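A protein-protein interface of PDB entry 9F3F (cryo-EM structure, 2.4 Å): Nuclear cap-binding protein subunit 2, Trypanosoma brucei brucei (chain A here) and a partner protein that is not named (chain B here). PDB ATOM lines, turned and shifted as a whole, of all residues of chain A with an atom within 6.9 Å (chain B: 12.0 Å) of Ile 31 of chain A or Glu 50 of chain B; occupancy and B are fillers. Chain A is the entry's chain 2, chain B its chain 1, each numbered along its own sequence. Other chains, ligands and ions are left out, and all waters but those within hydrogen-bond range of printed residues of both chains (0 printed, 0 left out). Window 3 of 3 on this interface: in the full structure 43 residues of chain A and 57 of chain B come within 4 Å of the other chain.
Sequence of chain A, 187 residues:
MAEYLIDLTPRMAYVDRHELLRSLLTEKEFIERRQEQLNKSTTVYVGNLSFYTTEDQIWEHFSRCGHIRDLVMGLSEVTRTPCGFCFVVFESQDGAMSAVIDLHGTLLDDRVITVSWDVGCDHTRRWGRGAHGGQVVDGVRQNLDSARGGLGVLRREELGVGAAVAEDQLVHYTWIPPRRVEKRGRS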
ATOM      1  N   THR A   9     -17.092  17.067 -16.558  1.00  0.00           N
ATOM      2  CA  THR A   9     -16.267  17.701 -17.614  1.00  0.00           C
ATOM      3  C   THR A   9     -17.184  18.578 -18.462  1.00  0.00           C
ATOM      4  O   THR A   9     -18.223  18.098 -18.918  1.00  0.00           O
ATOM      5  CB  THR A   9     -15.487  16.659 -18.423  1.00  0.00           C
ATOM      6  OG1 THR A   9     -14.578  16.015 -17.531  1.00  0.00           O
ATOM      7  CG2 THR A   9     -14.725  17.257 -19.584  1.00  0.00           C
ATOM      8  N   PRO A  10     -16.819  19.854 -18.677  1.00  0.00           N
ATOM      9  CA  PRO A  10     -17.598  20.741 -19.509  1.00  0.00           C
ATOM     10  C   PRO A  10     -17.712  20.259 -20.950  1.00  0.00           C
ATOM     11  O   PRO A  10     -16.700  20.197 -21.607  1.00  0.00           O
ATOM     12  CB  PRO A  10     -16.737  22.000 -19.481  1.00  0.00           C
ATOM     13  CG  PRO A  10     -16.044  21.951 -18.155  1.00  0.00           C
ATOM     14  CD  PRO A  10     -15.662  20.497 -18.053  1.00  0.00           C
ATOM     15  N   ARG A  11     -18.915  19.918 -21.399  1.00  0.00           N
ATOM     16  CA  ARG A  11     -19.121  19.532 -22.821  1.00  0.00           C
ATOM     17  C   ARG A  11     -20.308  20.299 -23.406  1.00  0.00           C
ATOM     18  O   ARG A  11     -21.392  20.243 -22.812  1.00  0.00           O
ATOM     19  CB  ARG A  11     -19.197  18.007 -22.939  1.00  0.00           C
ATOM     20  CG  ARG A  11     -17.853  17.341 -22.691  1.00  0.00           C
ATOM     21  CD  ARG A  11     -17.767  15.831 -22.710  1.00  0.00           C
ATOM     22  NE  ARG A  11     -18.380  15.145 -21.590  1.00  0.00           N
ATOM     23  CZ  ARG A  11     -17.700  14.359 -20.766  1.00  0.00           C
ATOM     24  NH1 ARG A  11     -16.401  14.202 -20.935  1.00  0.00           N
ATOM     25  NH2 ARG A  11     -18.316  13.738 -19.776  1.00  0.00           N
ATOM     26  N   MET A  12     -20.097  20.978 -24.527  1.00  0.00           N
ATOM     27  CA  MET A  12     -21.160  21.773 -25.193  1.00  0.00           C
ATOM     28  C   MET A  12     -21.618  20.995 -26.430  1.00  0.00           C
ATOM     29  O   MET A  12     -20.785  20.787 -27.330  1.00  0.00           O
ATOM     30  CB  MET A  12     -20.598  23.136 -25.600  1.00  0.00           C
ATOM     31  CG  MET A  12     -21.329  23.795 -26.739  1.00  0.00           C
ATOM     32  SD  MET A  12     -20.557  25.383 -27.116  1.00  0.00           S
ATOM     33  CE  MET A  12     -19.825  25.756 -25.526  1.00  0.00           C
ATOM     34  N   ALA A  13     -22.875  20.549 -26.460  1.00  0.00           N
ATOM     35  CA  ALA A  13     -23.361  19.668 -27.549  1.00  0.00           C
ATOM     36  C   ALA A  13     -23.508  20.330 -28.919  1.00  0.00           C
ATOM     37  O   ALA A  13     -23.103  19.693 -29.906  1.00  0.00           O
ATOM     38  CB  ALA A  13     -24.680  19.076 -27.122  1.00  0.00           C
ATOM     39  N   VAL A  15     -23.381  22.966 -32.340  1.00  0.00           N
ATOM     40  CA  VAL A  15     -22.276  23.599 -33.119  1.00  0.00           C
ATOM     41  C   VAL A  15     -22.858  24.879 -33.720  1.00  0.00           C
ATOM     42  O   VAL A  15     -24.093  24.939 -33.875  1.00  0.00           O
ATOM     43  CB  VAL A  15     -21.715  22.672 -34.208  1.00  0.00           C
ATOM     44  CG1 VAL A  15     -21.061  21.437 -33.607  1.00  0.00           C
ATOM     45  CG2 VAL A  15     -22.778  22.276 -35.219  1.00  0.00           C
ATOM     46  N   LEU A  24     -12.490  24.365 -39.999  1.00  0.00           N
ATOM     47  CA  LEU A  24     -11.926  23.250 -39.211  1.00  0.00           C
ATOM     48  C   LEU A  24     -12.884  22.067 -39.317  1.00  0.00           C
ATOM     49  O   LEU A  24     -14.063  22.285 -39.637  1.00  0.00           O
ATOM     50  CB  LEU A  24     -11.762  23.711 -37.762  1.00  0.00           C
ATOM     51  CG  LEU A  24     -10.659  24.731 -37.491  1.00  0.00           C
ATOM     52  CD1 LEU A  24     -10.474  24.935 -35.995  1.00  0.00           C
ATOM     53  CD2 LEU A  24      -9.348  24.295 -38.125  1.00  0.00           C
ATOM     54  N   LEU A  25     -12.382  20.859 -39.104  1.00  0.00           N
ATOM     55  CA  LEU A  25     -13.265  19.668 -39.076  1.00  0.00           C
ATOM     56  C   LEU A  25     -14.104  19.697 -37.794  1.00  0.00           C
ATOM     57  O   LEU A  25     -13.639  20.233 -36.784  1.00  0.00           O
ATOM     58  CB  LEU A  25     -12.390  18.412 -39.119  1.00  0.00           C
ATOM     59  CG  LEU A  25     -11.496  18.275 -40.350  1.00  0.00           C
ATOM     60  CD1 LEU A  25     -10.913  16.873 -40.439  1.00  0.00           C
ATOM     61  CD2 LEU A  25     -12.264  18.612 -41.618  1.00  0.00           C
ATOM     62  N   THR A  26     -15.320  19.168 -37.849  1.00  0.00           N
ATOM     63  CA  THR A  26     -16.157  19.083 -36.637  1.00  0.00           C
ATOM     64  C   THR A  26     -15.565  18.016 -35.740  1.00  0.00           C
ATOM     65  O   THR A  26     -16.181  17.707 -34.715  1.00  0.00           O
ATOM     66  CB  THR A  26     -17.585  18.653 -36.958  1.00  0.00           C
ATOM     67  OG1 THR A  26     -18.313  18.588 -35.733  1.00  0.00           O
ATOM     68  CG2 THR A  26     -17.650  17.313 -37.660  1.00  0.00           C
ATOM     69  N   GLU A  27     -14.452  17.435 -36.155  1.00  0.00           N
ATOM     70  CA  GLU A  27     -13.783  16.458 -35.266  1.00  0.00           C
ATOM     71  C   GLU A  27     -12.299  16.790 -35.185  1.00  0.00           C
ATOM     72  O   GLU A  27     -11.695  16.968 -36.258  1.00  0.00           O
ATOM     73  CB  GLU A  27     -13.979  15.031 -35.783  1.00  0.00           C
ATOM     74  CG  GLU A  27     -15.433  14.600 -35.840  1.00  0.00           C
ATOM     75  CD  GLU A  27     -15.656  13.190 -36.358  1.00  0.00           C
ATOM     76  OE1 GLU A  27     -16.828  12.768 -36.431  1.00  0.00           O
ATOM     77  OE2 GLU A  27     -14.659  12.517 -36.688  1.00  0.00           O
ATOM     78  N   LYS A  28     -11.758  16.942 -33.978  1.00  0.00           N
ATOM     79  CA  LYS A  28     -10.293  17.123 -33.793  1.00  0.00           C
ATOM     80  C   LYS A  28      -9.957  18.559 -34.174  1.00  0.00           C
ATOM     81  O   LYS A  28      -8.785  18.947 -34.063  1.00  0.00           O
ATOM     82  CB  LYS A  28      -9.485  16.089 -34.588  1.00  0.00           C
ATOM     83  CG  LYS A  28      -9.755  14.638 -34.217  1.00  0.00           C
ATOM     84  CD  LYS A  28      -9.500  14.342 -32.756  1.00  0.00           C
ATOM     85  CE  LYS A  28      -9.807  12.909 -32.379  1.00  0.00           C
ATOM     86  NZ  LYS A  28     -11.228  12.571 -32.632  1.00  0.00           N
ATOM     87  N   GLU A  29     -10.975  19.313 -34.571  1.00  0.00           N
ATOM     88  CA  GLU A  29     -10.737  20.745 -34.875  1.00  0.00           C
ATOM     89  C   GLU A  29     -11.729  21.583 -34.064  1.00  0.00           C
ATOM     90  O   GLU A  29     -11.364  21.968 -32.943  1.00  0.00           O
ATOM     91  CB  GLU A  29     -10.817  20.980 -36.383  1.00  0.00           C
ATOM     92  CG  GLU A  29      -9.744  20.257 -37.180  1.00  0.00           C
ATOM     93  CD  GLU A  29      -8.343  20.837 -37.077  1.00  0.00           C
ATOM     94  OE1 GLU A  29      -7.795  21.230 -38.125  1.00  0.00           O
ATOM     95  OE2 GLU A  29      -7.802  20.895 -35.956  1.00  0.00           O
ATOM     96  N   PHE A  30     -12.935  21.838 -34.582  1.00  0.00           N
ATOM     97  CA  PHE A  30     -13.821  22.699 -33.762  1.00  0.00           C
ATOM     98  C   PHE A  30     -14.153  21.979 -32.454  1.00  0.00           C
ATOM     99  O   PHE A  30     -14.043  22.603 -31.385  1.00  0.00           O
ATOM    100  CB  PHE A  30     -15.059  23.150 -34.534  1.00  0.00           C
ATOM    101  CG  PHE A  30     -16.188  23.576 -33.635  1.00  0.00           C
ATOM    102  CD1 PHE A  30     -15.995  24.547 -32.670  1.00  0.00           C
ATOM    103  CD2 PHE A  30     -17.444  23.008 -33.758  1.00  0.00           C
ATOM    104  CE1 PHE A  30     -17.025  24.922 -31.825  1.00  0.00           C
ATOM    105  CE2 PHE A  30     -18.480  23.401 -32.927  1.00  0.00           C
ATOM    106  CZ  PHE A  30     -18.271  24.361 -31.968  1.00  0.00           C
ATOM    107  N   ILE A  31     -14.489  20.699 -32.522  1.00  0.00           N
ATOM    108  CA  ILE A  31     -14.925  20.028 -31.268  1.00  0.00           C
ATOM    109  C   ILE A  31     -13.706  19.838 -30.357  1.00  0.00           C
ATOM    110  O   ILE A  31     -13.814  20.191 -29.168  1.00  0.00           O
ATOM    111  CB  ILE A  31     -15.713  18.731 -31.545  1.00  0.00           C
ATOM    112  CG1 ILE A  31     -16.677  18.394 -30.406  1.00  0.00           C
ATOM    113  CG2 ILE A  31     -14.787  17.567 -31.876  1.00  0.00           C
ATOM    114  CD1 ILE A  31     -17.482  17.138 -30.636  1.00  0.00           C
ATOM    115  N   GLU A  32     -12.588  19.338 -30.875  1.00  0.00           N
ATOM    116  CA  GLU A  32     -11.358  19.197 -30.046  1.00  0.00           C
ATOM    117  C   GLU A  32     -10.810  20.564 -29.612  1.00  0.00           C
ATOM    118  O   GLU A  32     -10.272  20.639 -28.501  1.00  0.00           O
ATOM    119  CB  GLU A  32     -10.302  18.360 -30.768  1.00  0.00           C
ATOM    120  CG  GLU A  32      -9.069  18.079 -29.929  1.00  0.00           C
ATOM    121  CD  GLU A  32      -8.026  17.217 -30.618  1.00  0.00           C
ATOM    122  OE1 GLU A  32      -7.522  17.634 -31.678  1.00  0.00           O
ATOM    123  OE2 GLU A  32      -7.724  16.127 -30.094  1.00  0.00           O
ATOM    124  N   ARG A  33     -10.833  21.579 -30.477  1.00  0.00           N
ATOM    125  CA  ARG A  33     -10.207  22.865 -30.065  1.00  0.00           C
ATOM    126  C   ARG A  33     -11.048  23.471 -28.937  1.00  0.00           C
ATOM    127  O   ARG A  33     -10.458  23.986 -27.965  1.00  0.00           O
ATOM    128  CB  ARG A  33     -10.067  23.835 -31.242  1.00  0.00           C
ATOM    129  CG  ARG A  33      -9.490  25.194 -30.879  1.00  0.00           C
ATOM    130  CD  ARG A  33      -9.344  26.008 -32.148  1.00  0.00           C
ATOM    131  NE  ARG A  33     -10.601  26.007 -32.880  1.00  0.00           N
ATOM    132  CZ  ARG A  33     -11.291  27.095 -33.197  1.00  0.00           C
ATOM    133  NH1 ARG A  33     -12.500  26.980 -33.717  1.00  0.00           N
ATOM    134  NH2 ARG A  33     -10.769  28.291 -32.988  1.00  0.00           N
ATOM    135  N   ARG A  34     -12.374  23.389 -29.066  1.00  0.00           N
ATOM    136  CA  ARG A  34     -13.258  23.958 -28.019  1.00  0.00           C
ATOM    137  C   ARG A  34     -12.995  23.241 -26.698  1.00  0.00           C
ATOM    138  O   ARG A  34     -13.108  23.908 -25.658  1.00  0.00           O
ATOM    139  CB  ARG A  34     -14.742  24.036 -28.400  1.00  0.00           C
ATOM    140  CG  ARG A  34     -15.519  22.732 -28.405  1.00  0.00           C
ATOM    141  CD  ARG A  34     -16.928  23.148 -28.774  1.00  0.00           C
ATOM    142  NE  ARG A  34     -17.851  22.050 -28.996  1.00  0.00           N
ATOM    143  CZ  ARG A  34     -19.112  22.216 -29.365  1.00  0.00           C
ATOM    144  NH1 ARG A  34     -19.618  23.433 -29.446  1.00  0.00           N
ATOM    145  NH2 ARG A  34     -19.863  21.168 -29.660  1.00  0.00           N
ATOM    146  N   GLN A  35     -12.683  21.954 -26.713  1.00  0.00           N
ATOM    147  CA  GLN A  35     -12.582  21.291 -25.392  1.00  0.00           C
ATOM    148  C   GLN A  35     -11.491  21.985 -24.572  1.00  0.00           C
ATOM    149  O   GLN A  35     -11.769  22.298 -23.409  1.00  0.00           O
ATOM    150  CB  GLN A  35     -12.417  19.774 -25.473  1.00  0.00           C
ATOM    151  CG  GLN A  35     -11.051  19.313 -25.957  1.00  0.00           C
ATOM    152  CD  GLN A  35     -10.995  17.818 -26.148  1.00  0.00           C
ATOM    153  OE1 GLN A  35     -11.977  17.109 -25.943  1.00  0.00           O
ATOM    154  NE2 GLN A  35      -9.837  17.327 -26.558  1.00  0.00           N
ATOM    155  N   GLU A  36     -10.353  22.339 -25.143  1.00  0.00           N
ATOM    156  CA  GLU A  36      -9.335  22.974 -24.265  1.00  0.00           C
ATOM    157  C   GLU A  36      -9.911  24.291 -23.724  1.00  0.00           C
ATOM    158  O   GLU A  36      -9.668  24.587 -22.545  1.00  0.00           O
ATOM    159  CB  GLU A  36      -8.005  23.110 -25.007  1.00  0.00           C
ATOM    160  CG  GLU A  36      -6.917  23.783 -24.190  1.00  0.00           C
ATOM    161  CD  GLU A  36      -6.436  23.028 -22.961  1.00  0.00           C
ATOM    162  OE1 GLU A  36      -5.559  23.562 -22.254  1.00  0.00           O
ATOM    163  OE2 GLU A  36      -6.922  21.905 -22.720  1.00  0.00           O
ATOM    164  N   LEU A  38     -13.261  25.113 -23.264  1.00  0.00           N
ATOM    165  CA  LEU A  38     -14.361  24.764 -22.328  1.00  0.00           C
ATOM    166  C   LEU A  38     -13.800  24.171 -21.048  1.00  0.00           C
ATOM    167  O   LEU A  38     -14.419  24.371 -19.990  1.00  0.00           O
ATOM    168  CB  LEU A  38     -15.265  23.716 -22.978  1.00  0.00           C
ATOM    169  CG  LEU A  38     -16.364  24.224 -23.903  1.00  0.00           C
ATOM    170  CD1 LEU A  38     -17.117  23.054 -24.506  1.00  0.00           C
ATOM    171  CD2 LEU A  38     -17.324  25.100 -23.122  1.00  0.00           C
ATOM    172  N   ASN A  39     -12.676  23.503 -21.128  1.00  0.00           N
ATOM    173  CA  ASN A  39     -12.142  22.778 -19.957  1.00  0.00           C
ATOM    174  C   ASN A  39     -11.593  23.845 -19.013  1.00  0.00           C
ATOM    175  O   ASN A  39     -11.345  23.543 -17.829  1.00  0.00           O
ATOM    176  CB  ASN A  39     -11.162  21.656 -20.320  1.00  0.00           C
ATOM    177  CG  ASN A  39     -11.808  20.496 -21.044  1.00  0.00           C
ATOM    178  OD1 ASN A  39     -11.372  20.105 -22.123  1.00  0.00           O
ATOM    179  ND2 ASN A  39     -12.795  19.882 -20.414  1.00  0.00           N
ATOM    180  N   TYR B  46     -12.270  10.511 -21.027  1.00  0.00           N
ATOM    181  CA  TYR B  46     -13.011  10.867 -19.786  1.00  0.00           C
ATOM    182  C   TYR B  46     -12.916  12.374 -19.571  1.00  0.00           C
ATOM    183  O   TYR B  46     -13.662  13.134 -20.225  1.00  0.00           O
ATOM    184  CB  TYR B  46     -12.436  10.133 -18.572  1.00  0.00           C
ATOM    185  CG  TYR B  46     -12.136   8.654 -18.772  1.00  0.00           C
ATOM    186  CD1 TYR B  46     -13.113   7.690 -18.561  1.00  0.00           C
ATOM    187  CD2 TYR B  46     -10.870   8.223 -19.150  1.00  0.00           C
ATOM    188  CE1 TYR B  46     -12.844   6.342 -18.734  1.00  0.00           C
ATOM    189  CE2 TYR B  46     -10.589   6.879 -19.325  1.00  0.00           C
ATOM    190  CZ  TYR B  46     -11.579   5.936 -19.117  1.00  0.00           C
ATOM    191  OH  TYR B  46     -11.308   4.610 -19.289  1.00  0.00           O
ATOM    192  N   GLY B  47     -12.022  12.797 -18.671  1.00  0.00           N
ATOM    193  CA  GLY B  47     -11.828  14.238 -18.411  1.00  0.00           C
ATOM    194  C   GLY B  47     -11.130  14.909 -19.577  1.00  0.00           C
ATOM    195  O   GLY B  47     -10.384  14.209 -20.296  1.00  0.00           O
ATOM    196  N   SER B  48     -11.439  16.176 -19.826  1.00  0.00           N
ATOM    197  CA  SER B  48     -10.762  16.932 -20.907  1.00  0.00           C
ATOM    198  C   SER B  48     -11.062  16.265 -22.244  1.00  0.00           C
ATOM    199  O   SER B  48     -10.206  16.331 -23.149  1.00  0.00           O
ATOM    200  CB  SER B  48      -9.278  17.030 -20.659  1.00  0.00           C
ATOM    201  OG  SER B  48      -8.635  17.735 -21.710  1.00  0.00           O
ATOM    202  N   SER B  49     -12.231  15.649 -22.354  1.00  0.00           N
ATOM    203  CA  SER B  49     -12.606  14.919 -23.594  1.00  0.00           C
ATOM    204  C   SER B  49     -13.984  15.403 -24.062  1.00  0.00           C
ATOM    205  O   SER B  49     -14.780  15.832 -23.201  1.00  0.00           O
ATOM    206  CB  SER B  49     -12.598  13.430 -23.372  1.00  0.00           C
ATOM    207  OG  SER B  49     -11.355  13.001 -22.832  1.00  0.00           O
ATOM    208  N   GLU B  50     -14.246  15.343 -25.371  1.00  0.00           N
ATOM    209  CA  GLU B  50     -15.565  15.766 -25.910  1.00  0.00           C
ATOM    210  C   GLU B  50     -16.566  14.606 -25.784  1.00  0.00           C
ATOM    211  O   GLU B  50     -17.780  14.859 -25.943  1.00  0.00           O
ATOM    212  CB  GLU B  50     -15.458  16.248 -27.358  1.00  0.00           C
ATOM    213  CG  GLU B  50     -15.074  17.720 -27.475  1.00  0.00           C
ATOM    214  CD  GLU B  50     -16.140  18.718 -27.055  1.00  0.00           C
ATOM    215  OE1 GLU B  50     -17.263  18.296 -26.705  1.00  0.00           O
ATOM    216  OE2 GLU B  50     -15.841  19.931 -27.071  1.00  0.00           O
ATOM    217  N   GLY B  51     -16.082  13.388 -25.510  1.00  0.00           N
ATOM    218  CA  GLY B  51     -16.992  12.277 -25.323  1.00  0.00           C
ATOM    219  C   GLY B  51     -16.675  11.508 -24.059  1.00  0.00           C
ATOM    220  O   GLY B  51     -15.504  11.314 -23.726  1.00  0.00           O
ATOM    221  N   ARG B  52     -17.733  11.086 -23.375  1.00  0.00           N
ATOM    222  CA  ARG B  52     -17.531  10.366 -22.095  1.00  0.00           C
ATOM    223  C   ARG B  52     -17.180   8.904 -22.359  1.00  0.00           C
ATOM    224  O   ARG B  52     -17.868   8.267 -23.175  1.00  0.00           O
ATOM    225  CB  ARG B  52     -18.777  10.412 -21.205  1.00  0.00           C
ATOM    226  CG  ARG B  52     -18.617   9.593 -19.931  1.00  0.00           C
ATOM    227  CD  ARG B  52     -19.853   9.457 -19.063  1.00  0.00           C
ATOM    228  NE  ARG B  52     -19.583   8.622 -17.901  1.00  0.00           N
ATOM    229  CZ  ARG B  52     -19.684   9.029 -16.642  1.00  0.00           C
ATOM    230  NH1 ARG B  52     -20.047  10.271 -16.376  1.00  0.00           N
ATOM    231  NH2 ARG B  52     -19.419   8.195 -15.652  1.00  0.00           N
ATOM    232  N   GLU B  53     -16.152   8.406 -21.686  1.00  0.00           N
ATOM    233  CA  GLU B  53     -15.798   6.999 -21.769  1.00  0.00           C
ATOM    234  C   GLU B  53     -16.262   6.262 -20.521  1.00  0.00           C
ATOM    235  O   GLU B  53     -16.157   6.777 -19.405  1.00  0.00           O
ATOM    236  CB  GLU B  53     -14.290   6.828 -21.950  1.00  0.00           C
ATOM    237  CG  GLU B  53     -13.656   7.872 -22.846  1.00  0.00           C
ATOM    238  CD  GLU B  53     -12.148   7.744 -22.908  1.00  0.00           C
ATOM    239  OE1 GLU B  53     -11.605   6.796 -22.304  1.00  0.00           O
ATOM    240  OE2 GLU B  53     -11.504   8.592 -23.559  1.00  0.00           O
ATOM    241  N   LEU B  54     -16.777   5.052 -20.720  1.00  0.00           N
ATOM    242  CA  LEU B  54     -17.270   4.242 -19.618  1.00  0.00           C
ATOM    243  C   LEU B  54     -16.110   3.788 -18.733  1.00  0.00           C
ATOM    244  O   LEU B  54     -14.933   3.886 -19.092  1.00  0.00           O
ATOM    245  CB  LEU B  54     -18.065   3.052 -20.155  1.00  0.00           C
ATOM    246  CG  LEU B  54     -17.530   2.314 -21.388  1.00  0.00           C
ATOM    247  CD1 LEU B  54     -16.392   1.362 -21.037  1.00  0.00           C
ATOM    248  CD2 LEU B  54     -18.654   1.570 -22.097  1.00  0.00           C
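NH1 of Arg 11 of chain A is in hydrogen-bond range of O of Tyr 46 of chain B, at 3.0 Å. The backbone carbonyl oxygen (O) of Ser 48 of chain B sits close to the side-chain amide oxygen (OE1) of Gln 35 of chain A (3.4 Å). The guanidinium group (NH1) of Arg 11 of chain A sits close to the backbone carbonyl oxygen (O) of Ser 49 of chain B (3.2 Å). NE of Arg 34 of chain A lies within salt-bridge range of OE2 of Glu 50 of chain B (3.5 Å). The backbone NH (N) of Glu 50 of chain B sits at hydrogen-bond distance from the side-chain amide oxygen (OE1) of Gln 35 of chain A (2.9 Å). O of Ile 31 of chain A lies close to OE2 of Glu 50 of chain B, 2.9 Å away.
The side-chain hydroxyl of Ser 49 of chain B is in hydrogen-bond range of the backbone NH of Tyr 46 of chain B. OE2 of Glu 53 of chain B lies within hydrogen-bond range of N of Tyr 46 of chain B. The backbone carbonyl oxygen (O) of Gly 47 of chain B sits at hydrogen-bond distance from the side-chain hydroxyl (OG) of Ser 49 of chain B (3.0 Å). O of Met 12 of chain A is in hydrogen-bond range of NH2 of Arg 34 of chain A. OD1 of Asn 39 of chain A lies close to O of Gln 35 of chain A.
Among the printed residues, merely in contact across the chains: Thr 9 of chain A with Gly 47 of chain B (3.4 Å), Thr 9 of chain A with Ser 48 of chain B (3.5 Å), Thr 9 of chain A with Ser 49 of chain B (3.9 Å), Arg 11 of chain A with Glu 50 of chain B (3.4 Å), Arg 11 of chain A with Arg 52 of chain B (3.6 Å), Gln 35 of chain A with Ser 49 of chain B (3.2 Å) and Asn 39 of chain A with Ser 48 of chain B (3.5 Å).
No residue of chain B comes within 4 Å of Ala 13 of chain A. No residue of chain B comes within 4 Å of Thr 26 of chain A. No residue of chain B comes within 4 Å of Glu 27 of chain A. No residue of chain B comes within 4 Å of Lys 28 of chain A. No residue of chain B comes within 4 Å of Phe 30 of chain A. Of chain B, only Glu 50 (2.9 Å) comes within 4 Å of Ile 31 of chain A. No residue of chain B comes within 4 Å of Glu 32 of chain A. Of chain B, only Ser 48, Ser 49 and Glu 50 come within 4 Å of Gln 35 of chain A. Of the printed residues of chain B, Asn 39 of chain A touches Ser 48. Printed residues of chain A within 4 Å of Tyr 46 of chain B: Arg 11. Printed residues of chain A within 4 Å of Gly 47 of chain B: Thr 9 (3.4 Å). Of the printed residues of chain A, Ser 49 of chain B touches Thr 9, Arg 11 and Gln 35. Glu 50 of chain B touches just these residues of chain A: Arg 11, Ile 31, Arg 34 and Gln 35. Leu 54 of chain B touches none of the printed residues of chain A. The nearest printed residue of chain A that does not touch Ser 48 of chain B is Glu 36 of chain A (4.6 Å).
Printed residues of chain A that touch a printed residue of chain B: Thr 9, Arg 11, Ile 31, Arg 34, Gln 35 and Asn 39. Hydrophobic or aromatic side chains of chain A that line the printed part of chain B: Ile 31. Of the 9 printed residues of chain B, 6 touch a printed residue of chain A. Among the printed residues, Asp or Glu carboxylates within 4 Å of a Lys or Arg side-chain nitrogen of the other chain: Arg 34 of chain A with Glu 50 of chain B (3.5 Å).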
